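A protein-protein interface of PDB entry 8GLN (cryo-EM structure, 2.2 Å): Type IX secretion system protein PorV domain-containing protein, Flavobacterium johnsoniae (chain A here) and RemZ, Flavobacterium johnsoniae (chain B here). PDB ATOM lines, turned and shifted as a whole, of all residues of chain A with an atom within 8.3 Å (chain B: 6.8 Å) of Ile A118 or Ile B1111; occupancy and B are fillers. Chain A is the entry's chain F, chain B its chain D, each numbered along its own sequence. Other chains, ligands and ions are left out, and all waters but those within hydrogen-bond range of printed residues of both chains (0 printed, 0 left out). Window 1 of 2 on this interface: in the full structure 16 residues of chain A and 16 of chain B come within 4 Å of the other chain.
O of Asp A88 lies within hydrogen-bond range of N of Gly A116 (3.4 Å). The backbone NH of Phe A115 is in hydrogen-bond range of the backbone carbonyl oxygen of Pro A135, at 3.4 Å. O of Val A133 lies within hydrogen-bond range of N of Ile A118 (2.7 Å). OE2 of Glu A119 is in salt-bridge range of NH2 of Arg A121 (3.0 Å). N of Leu A120 is in hydrogen-bond range of O of Arg A131, at 2.7 Å. The backbone carbonyl oxygen (O) of Ile B1111 is in hydrogen-bond range of the backbone NH (N) of Leu B1095 (2.7 Å).
Lys B1110 touches Asp A88. Ile B1096 touches Ile A89 (CD1 to CD1, 3.8 Å). CG2 of Ile A118 touches O of Lys B1110 (3.3 Å). Ile B1111 touches Ile A118 (CA to CG2, 3.8 Å). Val B1112 touches Ile A118 (CG2 to CG2, 3.8 Å). Leu A120 touches Val B1112. O of Val B1043 touches CD of Arg A121, at 3.5 Å. Ser B1044 touches Arg A121 (CA to O, 3.2 Å). Val A167 touches Val B1112 (CG1 to CG1, 3.9 Å).
Of chain B, only Lys B1110 (3.3 Å), Ile B1111 (3.8 Å) and Val B1112 (3.8 Å) come within 4 Å of Ile A118. Ile B1111 touches just one residue of chain A: Ile A118. Of the printed residues of chain A, Lys B1110 touches Asp A88 (3.6 Å), Phe A115 (2.4 Å) and Ile A118 (3.3 Å). Printed residues of chain A within 4 Å of Ser B1044: Arg A121 (3.2 Å). Of the printed residues of chain A, Val B1112 touches Ile A118 (3.8 Å), Leu A120 (3.6 Å) and Val A167 (3.9 Å). Printed residues of chain B within 4 Å of Ile A89: Ile B1096. Of the printed residues of chain B, Asp A88 touches Lys B1110 (3.6 Å). Phe B1113 touches none of the printed residues of chain A. The nearest residue of chain B that does not touch Ile A118 is Val B1094 (4.03 Å). The nearest printed residue of chain B that does not touch Arg A121 is Asn B1114 (5.6 Å).
O of Phe A115 sits at hydrogen-bond distance from NZ of Lys B1110 (2.4 Å). N of Val B1045 is in hydrogen-bond range of O of Arg A121, 3.2 Å away. The backbone NH of Val A167 lies within hydrogen-bond range of the side-chain amide oxygen of Gln B1093 (2.9 Å).
Among the printed residues, no Asp or Glu carboxylate lies within 4 Å of a Lys or Arg side-chain nitrogen of the other chain.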
ATOM      1  N   ASP A  88     -16.583  11.576 -32.616  1.00  0.00           N
ATOM      2  CA  ASP A  88     -16.761  12.412 -33.800  1.00  0.00           C
ATOM      3  C   ASP A  88     -15.452  12.956 -34.358  1.00  0.00           C
ATOM      4  O   ASP A  88     -15.479  13.862 -35.199  1.00  0.00           O
ATOM      5  CB  ASP A  88     -17.725  13.574 -33.535  1.00  0.00           C
ATOM      6  CG  ASP A  88     -19.162  13.115 -33.395  1.00  0.00           C
ATOM      7  OD1 ASP A  88     -19.745  12.669 -34.404  1.00  0.00           O
ATOM      8  OD2 ASP A  88     -19.711  13.199 -32.275  1.00  0.00           O
ATOM      9  N   ILE A  89     -14.311  12.440 -33.918  1.00  0.00           N
ATOM     10  CA  ILE A  89     -13.024  12.724 -34.540  1.00  0.00           C
ATOM     11  C   ILE A  89     -12.679  11.518 -35.400  1.00  0.00           C
ATOM     12  O   ILE A  89     -12.262  10.476 -34.885  1.00  0.00           O
ATOM     13  CB  ILE A  89     -11.930  12.997 -33.501  1.00  0.00           C
ATOM     14  CG1 ILE A  89     -12.387  14.067 -32.509  1.00  0.00           C
ATOM     15  CG2 ILE A  89     -10.638  13.409 -34.190  1.00  0.00           C
ATOM     16  CD1 ILE A  89     -11.355  14.397 -31.458  1.00  0.00           C
ATOM     17  N   GLY A 114     -12.384  15.244 -40.038  1.00  0.00           N
ATOM     18  CA  GLY A 114     -12.937  16.343 -39.279  1.00  0.00           C
ATOM     19  C   GLY A 114     -13.005  16.005 -37.804  1.00  0.00           C
ATOM     20  O   GLY A 114     -13.009  14.839 -37.406  1.00  0.00           O
ATOM     21  N   PHE A 115     -13.057  17.059 -36.995  1.00  0.00           N
ATOM     22  CA  PHE A 115     -13.191  16.936 -35.552  1.00  0.00           C
ATOM     23  C   PHE A 115     -14.634  17.074 -35.094  1.00  0.00           C
ATOM     24  O   PHE A 115     -14.894  17.080 -33.887  1.00  0.00           O
ATOM     25  CB  PHE A 115     -12.319  17.978 -34.854  1.00  0.00           C
ATOM     26  CG  PHE A 115     -10.871  17.892 -35.220  1.00  0.00           C
ATOM     27  CD1 PHE A 115     -10.066  16.904 -34.683  1.00  0.00           C
ATOM     28  CD2 PHE A 115     -10.314  18.795 -36.105  1.00  0.00           C
ATOM     29  CE1 PHE A 115      -8.734  16.820 -35.023  1.00  0.00           C
ATOM     30  CE2 PHE A 115      -8.982  18.717 -36.448  1.00  0.00           C
ATOM     31  CZ  PHE A 115      -8.191  17.727 -35.907  1.00  0.00           C
ATOM     32  N   GLY A 116     -15.573  17.184 -36.025  1.00  0.00           N
ATOM     33  CA  GLY A 116     -16.949  17.468 -35.677  1.00  0.00           C
ATOM     34  C   GLY A 116     -17.127  18.933 -35.319  1.00  0.00           C
ATOM     35  O   GLY A 116     -16.191  19.730 -35.318  1.00  0.00           O
ATOM     36  N   GLY A 117     -18.371  19.284 -35.013  1.00  0.00           N
ATOM     37  CA  GLY A 117     -18.667  20.647 -34.605  1.00  0.00           C
ATOM     38  C   GLY A 117     -18.032  20.958 -33.262  1.00  0.00           C
ATOM     39  O   GLY A 117     -18.143  20.176 -32.310  1.00  0.00           O
ATOM     40  N   ILE A 118     -17.358  22.099 -33.180  1.00  0.00           N
ATOM     41  CA  ILE A 118     -16.768  22.584 -31.939  1.00  0.00           C
ATOM     42  C   ILE A 118     -17.390  23.935 -31.626  1.00  0.00           C
ATOM     43  O   ILE A 118     -17.369  24.844 -32.466  1.00  0.00           O
ATOM     44  CB  ILE A 118     -15.237  22.692 -32.028  1.00  0.00           C
ATOM     45  CG1 ILE A 118     -14.634  21.371 -32.509  1.00  0.00           C
ATOM     46  CG2 ILE A 118     -14.657  23.094 -30.683  1.00  0.00           C
ATOM     47  CD1 ILE A 118     -13.195  21.485 -32.945  1.00  0.00           C
ATOM     48  N   GLU A 119     -17.935  24.068 -30.423  1.00  0.00           N
ATOM     49  CA  GLU A 119     -18.591  25.300 -30.014  1.00  0.00           C
ATOM     50  C   GLU A 119     -17.561  26.291 -29.487  1.00  0.00           C
ATOM     51  O   GLU A 119     -16.769  25.963 -28.599  1.00  0.00           O
ATOM     52  CB  GLU A 119     -19.641  25.004 -28.945  1.00  0.00           C
ATOM     53  CG  GLU A 119     -20.553  26.169 -28.624  1.00  0.00           C
ATOM     54  CD  GLU A 119     -21.759  25.757 -27.805  1.00  0.00           C
ATOM     55  OE1 GLU A 119     -21.641  24.799 -27.011  1.00  0.00           O
ATOM     56  OE2 GLU A 119     -22.825  26.390 -27.954  1.00  0.00           O
ATOM     57  N   LEU A 120     -17.568  27.504 -30.040  1.00  0.00           N
ATOM     58  CA  LEU A 120     -16.676  28.568 -29.585  1.00  0.00           C
ATOM     59  C   LEU A 120     -17.428  29.414 -28.564  1.00  0.00           C
ATOM     60  O   LEU A 120     -17.916  30.507 -28.849  1.00  0.00           O
ATOM     61  CB  LEU A 120     -16.173  29.404 -30.754  1.00  0.00           C
ATOM     62  CG  LEU A 120     -15.493  28.648 -31.892  1.00  0.00           C
ATOM     63  CD1 LEU A 120     -14.733  29.619 -32.768  1.00  0.00           C
ATOM     64  CD2 LEU A 120     -14.564  27.590 -31.342  1.00  0.00           C
ATOM     65  N   ARG A 121     -17.513  28.887 -27.349  1.00  0.00           N
ATOM     66  CA  ARG A 121     -18.189  29.567 -26.250  1.00  0.00           C
ATOM     67  C   ARG A 121     -17.166  30.460 -25.562  1.00  0.00           C
ATOM     68  O   ARG A 121     -16.245  29.975 -24.901  1.00  0.00           O
ATOM     69  CB  ARG A 121     -18.800  28.551 -25.293  1.00  0.00           C
ATOM     70  CG  ARG A 121     -19.455  29.156 -24.076  1.00  0.00           C
ATOM     71  CD  ARG A 121     -20.119  28.082 -23.238  1.00  0.00           C
ATOM     72  NE  ARG A 121     -21.093  27.326 -24.014  1.00  0.00           N
ATOM     73  CZ  ARG A 121     -22.319  27.749 -24.291  1.00  0.00           C
ATOM     74  NH1 ARG A 121     -22.757  28.922 -23.863  1.00  0.00           N
ATOM     75  NH2 ARG A 121     -23.125  26.976 -25.012  1.00  0.00           N
ATOM     76  N   THR A 130     -23.538  31.155 -29.901  1.00  0.00           N
ATOM     77  CA  THR A 130     -22.190  30.625 -30.026  1.00  0.00           C
ATOM     78  C   THR A 130     -21.881  30.285 -31.476  1.00  0.00           C
ATOM     79  O   THR A 130     -22.692  29.661 -32.167  1.00  0.00           O
ATOM     80  CB  THR A 130     -22.010  29.376 -29.160  1.00  0.00           C
ATOM     81  OG1 THR A 130     -23.170  28.543 -29.268  1.00  0.00           O
ATOM     82  CG2 THR A 130     -21.804  29.759 -27.707  1.00  0.00           C
ATOM     83  N   ARG A 131     -20.706  30.708 -31.928  1.00  0.00           N
ATOM     84  CA  ARG A 131     -20.190  30.289 -33.222  1.00  0.00           C
ATOM     85  C   ARG A 131     -19.661  28.864 -33.131  1.00  0.00           C
ATOM     86  O   ARG A 131     -18.926  28.519 -32.203  1.00  0.00           O
ATOM     87  CB  ARG A 131     -19.084  31.240 -33.679  1.00  0.00           C
ATOM     88  CG  ARG A 131     -18.372  30.823 -34.950  1.00  0.00           C
ATOM     89  CD  ARG A 131     -17.569  31.978 -35.533  1.00  0.00           C
ATOM     90  NE  ARG A 131     -16.487  32.406 -34.655  1.00  0.00           N
ATOM     91  CZ  ARG A 131     -15.198  32.230 -34.915  1.00  0.00           C
ATOM     92  NH1 ARG A 131     -14.791  31.624 -36.019  1.00  0.00           N
ATOM     93  NH2 ARG A 131     -14.295  32.673 -34.046  1.00  0.00           N
ATOM     94  N   GLU A 132     -20.048  28.032 -34.093  1.00  0.00           N
ATOM     95  CA  GLU A 132     -19.572  26.658 -34.174  1.00  0.00           C
ATOM     96  C   GLU A 132     -18.643  26.515 -35.369  1.00  0.00           C
ATOM     97  O   GLU A 132     -18.986  26.930 -36.482  1.00  0.00           O
ATOM     98  CB  GLU A 132     -20.733  25.668 -34.289  1.00  0.00           C
ATOM     99  CG  GLU A 132     -20.311  24.216 -34.106  1.00  0.00           C
ATOM    100  CD  GLU A 132     -21.481  23.285 -33.860  1.00  0.00           C
ATOM    101  OE1 GLU A 132     -21.946  22.643 -34.826  1.00  0.00           O
ATOM    102  OE2 GLU A 132     -21.935  23.190 -32.700  1.00  0.00           O
ATOM    103  N   VAL A 133     -17.474  25.934 -35.136  1.00  0.00           N
ATOM    104  CA  VAL A 133     -16.499  25.688 -36.188  1.00  0.00           C
ATOM    105  C   VAL A 133     -16.309  24.187 -36.333  1.00  0.00           C
ATOM    106  O   VAL A 133     -16.415  23.428 -35.365  1.00  0.00           O
ATOM    107  CB  VAL A 133     -15.151  26.387 -35.908  1.00  0.00           C
ATOM    108  CG1 VAL A 133     -15.340  27.890 -35.867  1.00  0.00           C
ATOM    109  CG2 VAL A 133     -14.551  25.888 -34.604  1.00  0.00           C
ATOM    110  N   ASN A 134     -16.042  23.759 -37.562  1.00  0.00           N
ATOM    111  CA  ASN A 134     -15.757  22.361 -37.871  1.00  0.00           C
ATOM    112  C   ASN A 134     -14.445  22.309 -38.641  1.00  0.00           C
ATOM    113  O   ASN A 134     -14.431  22.234 -39.877  1.00  0.00           O
ATOM    114  CB  ASN A 134     -16.919  21.712 -38.631  1.00  0.00           C
ATOM    115  CG  ASN A 134     -17.243  22.419 -39.935  1.00  0.00           C
ATOM    116  OD1 ASN A 134     -17.336  23.644 -39.983  1.00  0.00           O
ATOM    117  ND2 ASN A 134     -17.417  21.644 -40.999  1.00  0.00           N
ATOM    118  N   PRO A 135     -13.314  22.370 -37.939  1.00  0.00           N
ATOM    119  CA  PRO A 135     -12.021  22.216 -38.617  1.00  0.00           C
ATOM    120  C   PRO A 135     -11.964  20.873 -39.325  1.00  0.00           C
ATOM    121  O   PRO A 135     -12.306  19.835 -38.755  1.00  0.00           O
ATOM    122  CB  PRO A 135     -11.001  22.302 -37.476  1.00  0.00           C
ATOM    123  CG  PRO A 135     -11.730  22.922 -36.337  1.00  0.00           C
ATOM    124  CD  PRO A 135     -13.165  22.541 -36.485  1.00  0.00           C
ATOM    125  N   ASN A 136     -11.534  20.897 -40.581  1.00  0.00           N
ATOM    126  CA  ASN A 136     -11.627  19.692 -41.387  1.00  0.00           C
ATOM    127  C   ASN A 136     -10.636  19.757 -42.535  1.00  0.00           C
ATOM    128  O   ASN A 136     -10.123  20.821 -42.886  1.00  0.00           O
ATOM    129  CB  ASN A 136     -13.049  19.488 -41.921  1.00  0.00           C
ATOM    130  CG  ASN A 136     -13.468  20.572 -42.893  1.00  0.00           C
ATOM    131  OD1 ASN A 136     -13.358  20.406 -44.107  1.00  0.00           O
ATOM    132  ND2 ASN A 136     -13.952  21.687 -42.363  1.00  0.00           N
ATOM    133  N   LEU A 165      -8.084  23.340 -41.309  1.00  0.00           N
ATOM    134  CA  LEU A 165      -7.940  22.975 -39.905  1.00  0.00           C
ATOM    135  C   LEU A 165      -7.825  24.182 -38.984  1.00  0.00           C
ATOM    136  O   LEU A 165      -8.095  24.053 -37.785  1.00  0.00           O
ATOM    137  CB  LEU A 165      -6.715  22.076 -39.723  1.00  0.00           C
ATOM    138  CG  LEU A 165      -6.749  20.730 -40.450  1.00  0.00           C
ATOM    139  CD1 LEU A 165      -5.520  19.908 -40.104  1.00  0.00           C
ATOM    140  CD2 LEU A 165      -8.019  19.968 -40.111  1.00  0.00           C
ATOM    141  N   VAL A 167      -8.592  27.674 -37.041  1.00  0.00           N
ATOM    142  CA  VAL A 167      -9.753  28.380 -36.515  1.00  0.00           C
ATOM    143  C   VAL A 167      -9.426  29.866 -36.464  1.00  0.00           C
ATOM    144  O   VAL A 167      -8.337  30.258 -36.030  1.00  0.00           O
ATOM    145  CB  VAL A 167     -10.154  27.853 -35.125  1.00  0.00           C
ATOM    146  CG1 VAL A 167     -11.446  28.502 -34.662  1.00  0.00           C
ATOM    147  CG2 VAL A 167     -10.295  26.336 -35.157  1.00  0.00           C
ATOM    148  N   VAL B1043     -18.010  24.825 -21.093  1.00  0.00           N
ATOM    149  CA  VAL B1043     -16.593  25.166 -21.106  1.00  0.00           C
ATOM    150  C   VAL B1043     -16.427  26.433 -21.930  1.00  0.00           C
ATOM    151  O   VAL B1043     -16.944  26.524 -23.049  1.00  0.00           O
ATOM    152  CB  VAL B1043     -15.729  24.027 -21.679  1.00  0.00           C
ATOM    153  CG1 VAL B1043     -14.259  24.352 -21.511  1.00  0.00           C
ATOM    154  CG2 VAL B1043     -16.065  22.714 -21.004  1.00  0.00           C
ATOM    155  N   SER B1044     -15.711  27.410 -21.379  1.00  0.00           N
ATOM    156  CA  SER B1044     -15.496  28.682 -22.047  1.00  0.00           C
ATOM    157  C   SER B1044     -14.018  29.043 -22.017  1.00  0.00           C
ATOM    158  O   SER B1044     -13.306  28.740 -21.057  1.00  0.00           O
ATOM    159  CB  SER B1044     -16.323  29.799 -21.403  1.00  0.00           C
ATOM    160  OG  SER B1044     -15.951  29.995 -20.051  1.00  0.00           O
ATOM    161  N   VAL B1045     -13.564  29.692 -23.087  1.00  0.00           N
ATOM    162  CA  VAL B1045     -12.190  30.166 -23.217  1.00  0.00           C
ATOM    163  C   VAL B1045     -12.257  31.628 -23.636  1.00  0.00           C
ATOM    164  O   VAL B1045     -12.790  31.941 -24.706  1.00  0.00           O
ATOM    165  CB  VAL B1045     -11.384  29.348 -24.236  1.00  0.00           C
ATOM    166  CG1 VAL B1045      -9.927  29.774 -24.223  1.00  0.00           C
ATOM    167  CG2 VAL B1045     -11.512  27.861 -23.953  1.00  0.00           C
ATOM    168  N   ILE B1050      -9.260  28.724 -19.484  1.00  0.00           N
ATOM    169  CA  ILE B1050     -10.372  27.798 -19.650  1.00  0.00           C
ATOM    170  C   ILE B1050     -11.204  27.821 -18.378  1.00  0.00           C
ATOM    171  O   ILE B1050     -10.677  27.618 -17.278  1.00  0.00           O
ATOM    172  CB  ILE B1050      -9.881  26.375 -19.964  1.00  0.00           C
ATOM    173  CG1 ILE B1050      -9.013  26.378 -21.221  1.00  0.00           C
ATOM    174  CG2 ILE B1050     -11.056  25.440 -20.147  1.00  0.00           C
ATOM    175  CD1 ILE B1050      -8.181  25.134 -21.384  1.00  0.00           C
ATOM    176  N   ILE B1064      -7.116  17.757 -19.546  1.00  0.00           N
ATOM    177  CA  ILE B1064      -7.160  18.463 -20.820  1.00  0.00           C
ATOM    178  C   ILE B1064      -6.153  17.821 -21.760  1.00  0.00           C
ATOM    179  O   ILE B1064      -4.973  17.680 -21.419  1.00  0.00           O
ATOM    180  CB  ILE B1064      -6.871  19.963 -20.637  1.00  0.00           C
ATOM    181  CG1 ILE B1064      -7.950  20.608 -19.766  1.00  0.00           C
ATOM    182  CG2 ILE B1064      -6.785  20.660 -21.983  1.00  0.00           C
ATOM    183  CD1 ILE B1064      -7.538  21.927 -19.166  1.00  0.00           C
ATOM    184  N   PHE B1088      -2.568  27.121 -17.043  1.00  0.00           N
ATOM    185  CA  PHE B1088      -2.366  26.338 -18.251  1.00  0.00           C
ATOM    186  C   PHE B1088      -2.469  27.244 -19.467  1.00  0.00           C
ATOM    187  O   PHE B1088      -3.345  28.111 -19.531  1.00  0.00           O
ATOM    188  CB  PHE B1088      -3.391  25.199 -18.346  1.00  0.00           C
ATOM    189  CG  PHE B1088      -3.518  24.607 -19.717  1.00  0.00           C
ATOM    190  CD1 PHE B1088      -2.575  23.711 -20.189  1.00  0.00           C
ATOM    191  CD2 PHE B1088      -4.588  24.935 -20.530  1.00  0.00           C
ATOM    192  CE1 PHE B1088      -2.691  23.163 -21.446  1.00  0.00           C
ATOM    193  CE2 PHE B1088      -4.708  24.389 -21.789  1.00  0.00           C
ATOM    194  CZ  PHE B1088      -3.760  23.501 -22.247  1.00  0.00           C
ATOM    195  N   GLN B1093      -4.815  25.541 -30.430  1.00  0.00           N
ATOM    196  CA  GLN B1093      -6.176  25.512 -30.960  1.00  0.00           C
ATOM    197  C   GLN B1093      -7.048  24.455 -30.289  1.00  0.00           C
ATOM    198  O   GLN B1093      -7.585  24.690 -29.204  1.00  0.00           O
ATOM    199  CB  GLN B1093      -6.155  25.299 -32.478  1.00  0.00           C
ATOM    200  CG  GLN B1093      -5.319  26.320 -33.236  1.00  0.00           C
ATOM    201  CD  GLN B1093      -6.159  27.237 -34.105  1.00  0.00           C
ATOM    202  OE1 GLN B1093      -6.537  26.879 -35.220  1.00  0.00           O
ATOM    203  NE2 GLN B1093      -6.455  28.427 -33.598  1.00  0.00           N
ATOM    204  N   VAL B1094      -7.193  23.294 -30.918  1.00  0.00           N
ATOM    205  CA  VAL B1094      -8.227  22.341 -30.522  1.00  0.00           C
ATOM    206  C   VAL B1094      -7.758  21.540 -29.313  1.00  0.00           C
ATOM    207  O   VAL B1094      -6.667  20.959 -29.318  1.00  0.00           O
ATOM    208  CB  VAL B1094      -8.593  21.419 -31.694  1.00  0.00           C
ATOM    209  CG1 VAL B1094      -9.524  20.314 -31.229  1.00  0.00           C
ATOM    210  CG2 VAL B1094      -9.233  22.222 -32.812  1.00  0.00           C
ATOM    211  N   LEU B1095      -8.594  21.505 -28.277  1.00  0.00           N
ATOM    212  CA  LEU B1095      -8.330  20.761 -27.055  1.00  0.00           C
ATOM    213  C   LEU B1095      -9.554  19.939 -26.685  1.00  0.00           C
ATOM    214  O   LEU B1095     -10.685  20.288 -27.032  1.00  0.00           O
ATOM    215  CB  LEU B1095      -7.973  21.694 -25.892  1.00  0.00           C
ATOM    216  CG  LEU B1095      -6.642  22.433 -25.983  1.00  0.00           C
ATOM    217  CD1 LEU B1095      -6.354  23.161 -24.688  1.00  0.00           C
ATOM    218  CD2 LEU B1095      -5.538  21.446 -26.289  1.00  0.00           C
ATOM    219  N   ILE B1096      -9.319  18.841 -25.974  1.00  0.00           N
ATOM    220  CA  ILE B1096     -10.381  17.978 -25.472  1.00  0.00           C
ATOM    221  C   ILE B1096     -10.363  18.048 -23.954  1.00  0.00           C
ATOM    222  O   ILE B1096      -9.351  17.718 -23.322  1.00  0.00           O
ATOM    223  CB  ILE B1096     -10.221  16.530 -25.956  1.00  0.00           C
ATOM    224  CG1 ILE B1096     -10.253  16.470 -27.482  1.00  0.00           C
ATOM    225  CG2 ILE B1096     -11.310  15.653 -25.366  1.00  0.00           C
ATOM    226  CD1 ILE B1096      -9.892  15.119 -28.039  1.00  0.00           C
ATOM    227  N   VAL B1097     -11.475  18.474 -23.370  1.00  0.00           N
ATOM    228  CA  VAL B1097     -11.620  18.561 -21.924  1.00  0.00           C
ATOM    229  C   VAL B1097     -12.463  17.383 -21.463  1.00  0.00           C
ATOM    230  O   VAL B1097     -13.606  17.214 -21.905  1.00  0.00           O
ATOM    231  CB  VAL B1097     -12.256  19.894 -21.500  1.00  0.00           C
ATOM    232  CG1 VAL B1097     -12.264  20.016 -19.988  1.00  0.00           C
ATOM    233  CG2 VAL B1097     -11.511  21.058 -22.129  1.00  0.00           C
ATOM    234  N   LYS B1109     -15.829  17.436 -23.664  1.00  0.00           N
ATOM    235  CA  LYS B1109     -16.106  18.636 -24.440  1.00  0.00           C
ATOM    236  C   LYS B1109     -14.886  18.985 -25.278  1.00  0.00           C
ATOM    237  O   LYS B1109     -13.761  18.995 -24.770  1.00  0.00           O
ATOM    238  CB  LYS B1109     -16.478  19.810 -23.530  1.00  0.00           C
ATOM    239  CG  LYS B1109     -17.285  20.897 -24.220  1.00  0.00           C
ATOM    240  CD  LYS B1109     -18.758  20.524 -24.335  1.00  0.00           C
ATOM    241  CE  LYS B1109     -19.269  19.855 -23.070  1.00  0.00           C
ATOM    242  NZ  LYS B1109     -20.758  19.855 -23.003  1.00  0.00           N
ATOM    243  N   LYS B1110     -15.112  19.268 -26.557  1.00  0.00           N
ATOM    244  CA  LYS B1110     -14.066  19.733 -27.455  1.00  0.00           C
ATOM    245  C   LYS B1110     -14.101  21.254 -27.503  1.00  0.00           C
ATOM    246  O   LYS B1110     -15.171  21.847 -27.666  1.00  0.00           O
ATOM    247  CB  LYS B1110     -14.244  19.153 -28.859  1.00  0.00           C
ATOM    248  CG  LYS B1110     -13.921  17.675 -28.961  1.00  0.00           C
ATOM    249  CD  LYS B1110     -14.137  17.153 -30.372  1.00  0.00           C
ATOM    250  CE  LYS B1110     -15.601  16.839 -30.621  1.00  0.00           C
ATOM    251  NZ  LYS B1110     -15.799  16.066 -31.875  1.00  0.00           N
ATOM    252  N   ILE B1111     -12.935  21.879 -27.351  1.00  0.00           N
ATOM    253  CA  ILE B1111     -12.833  23.330 -27.316  1.00  0.00           C
ATOM    254  C   ILE B1111     -11.712  23.778 -28.240  1.00  0.00           C
ATOM    255  O   ILE B1111     -10.837  23.000 -28.623  1.00  0.00           O
ATOM    256  CB  ILE B1111     -12.586  23.865 -25.889  1.00  0.00           C
ATOM    257  CG1 ILE B1111     -11.284  23.296 -25.326  1.00  0.00           C
ATOM    258  CG2 ILE B1111     -13.755  23.532 -24.983  1.00  0.00           C
ATOM    259  CD1 ILE B1111     -10.650  24.159 -24.266  1.00  0.00           C
ATOM    260  N   VAL B1112     -11.751  25.058 -28.594  1.00  0.00           N
ATOM    261  CA  VAL B1112     -10.686  25.711 -29.341  1.00  0.00           C
ATOM    262  C   VAL B1112     -10.018  26.700 -28.400  1.00  0.00           C
ATOM    263  O   VAL B1112     -10.678  27.590 -27.850  1.00  0.00           O
ATOM    264  CB  VAL B1112     -11.215  26.408 -30.602  1.00  0.00           C
ATOM    265  CG1 VAL B1112     -10.131  27.270 -31.224  1.00  0.00           C
ATOM    266  CG2 VAL B1112     -11.714  25.377 -31.600  1.00  0.00           C
ATOM    267  N   PHE B1113      -8.709  26.542 -28.206  1.00  0.00           N
ATOM    268  CA  PHE B1113      -7.982  27.335 -27.218  1.00  0.00           C
ATOM    269  C   PHE B1113      -7.627  28.681 -27.843  1.00  0.00           C
ATOM    270  O   PHE B1113      -6.548  28.886 -28.404  1.00  0.00           O
ATOM    271  CB  PHE B1113      -6.746  26.590 -26.736  1.00  0.00           C
ATOM    272  CG  PHE B1113      -6.204  27.101 -25.439  1.00  0.00           C
ATOM    273  CD1 PHE B1113      -4.847  27.067 -25.176  1.00  0.00           C
ATOM    274  CD2 PHE B1113      -7.057  27.603 -24.473  1.00  0.00           C
ATOM    275  CE1 PHE B1113      -4.353  27.536 -23.978  1.00  0.00           C
ATOM    276  CE2 PHE B1113      -6.569  28.071 -23.274  1.00  0.00           C
ATOM    277  CZ  PHE B1113      -5.215  28.036 -23.026  1.00  0.00           C
ATOM    278  N   ASN B1114      -8.568  29.615 -27.743  1.00  0.00           N
ATOM    279  CA  ASN B1114      -8.391  30.953 -28.297  1.00  0.00           C
ATOM    280  C   ASN B1114      -7.304  31.718 -27.550  1.00  0.00           C
ATOM    281  O   ASN B1114      -6.985  31.408 -26.403  1.00  0.00           O
ATOM    282  CB  ASN B1114      -9.707  31.733 -28.248  1.00  0.00           C
ATOM    283  CG  ASN B1114     -10.826  31.040 -28.999  1.00  0.00           C
ATOM    284  OD1 ASN B1114     -10.846  31.023 -30.230  1.00  0.00           O
ATOM    285  ND2 ASN B1114     -11.764  30.461 -28.260  1.00  0.00           N
ATOM    286  OXT ASN B1114      -6.720  32.667 -28.075  1.00  0.00           O
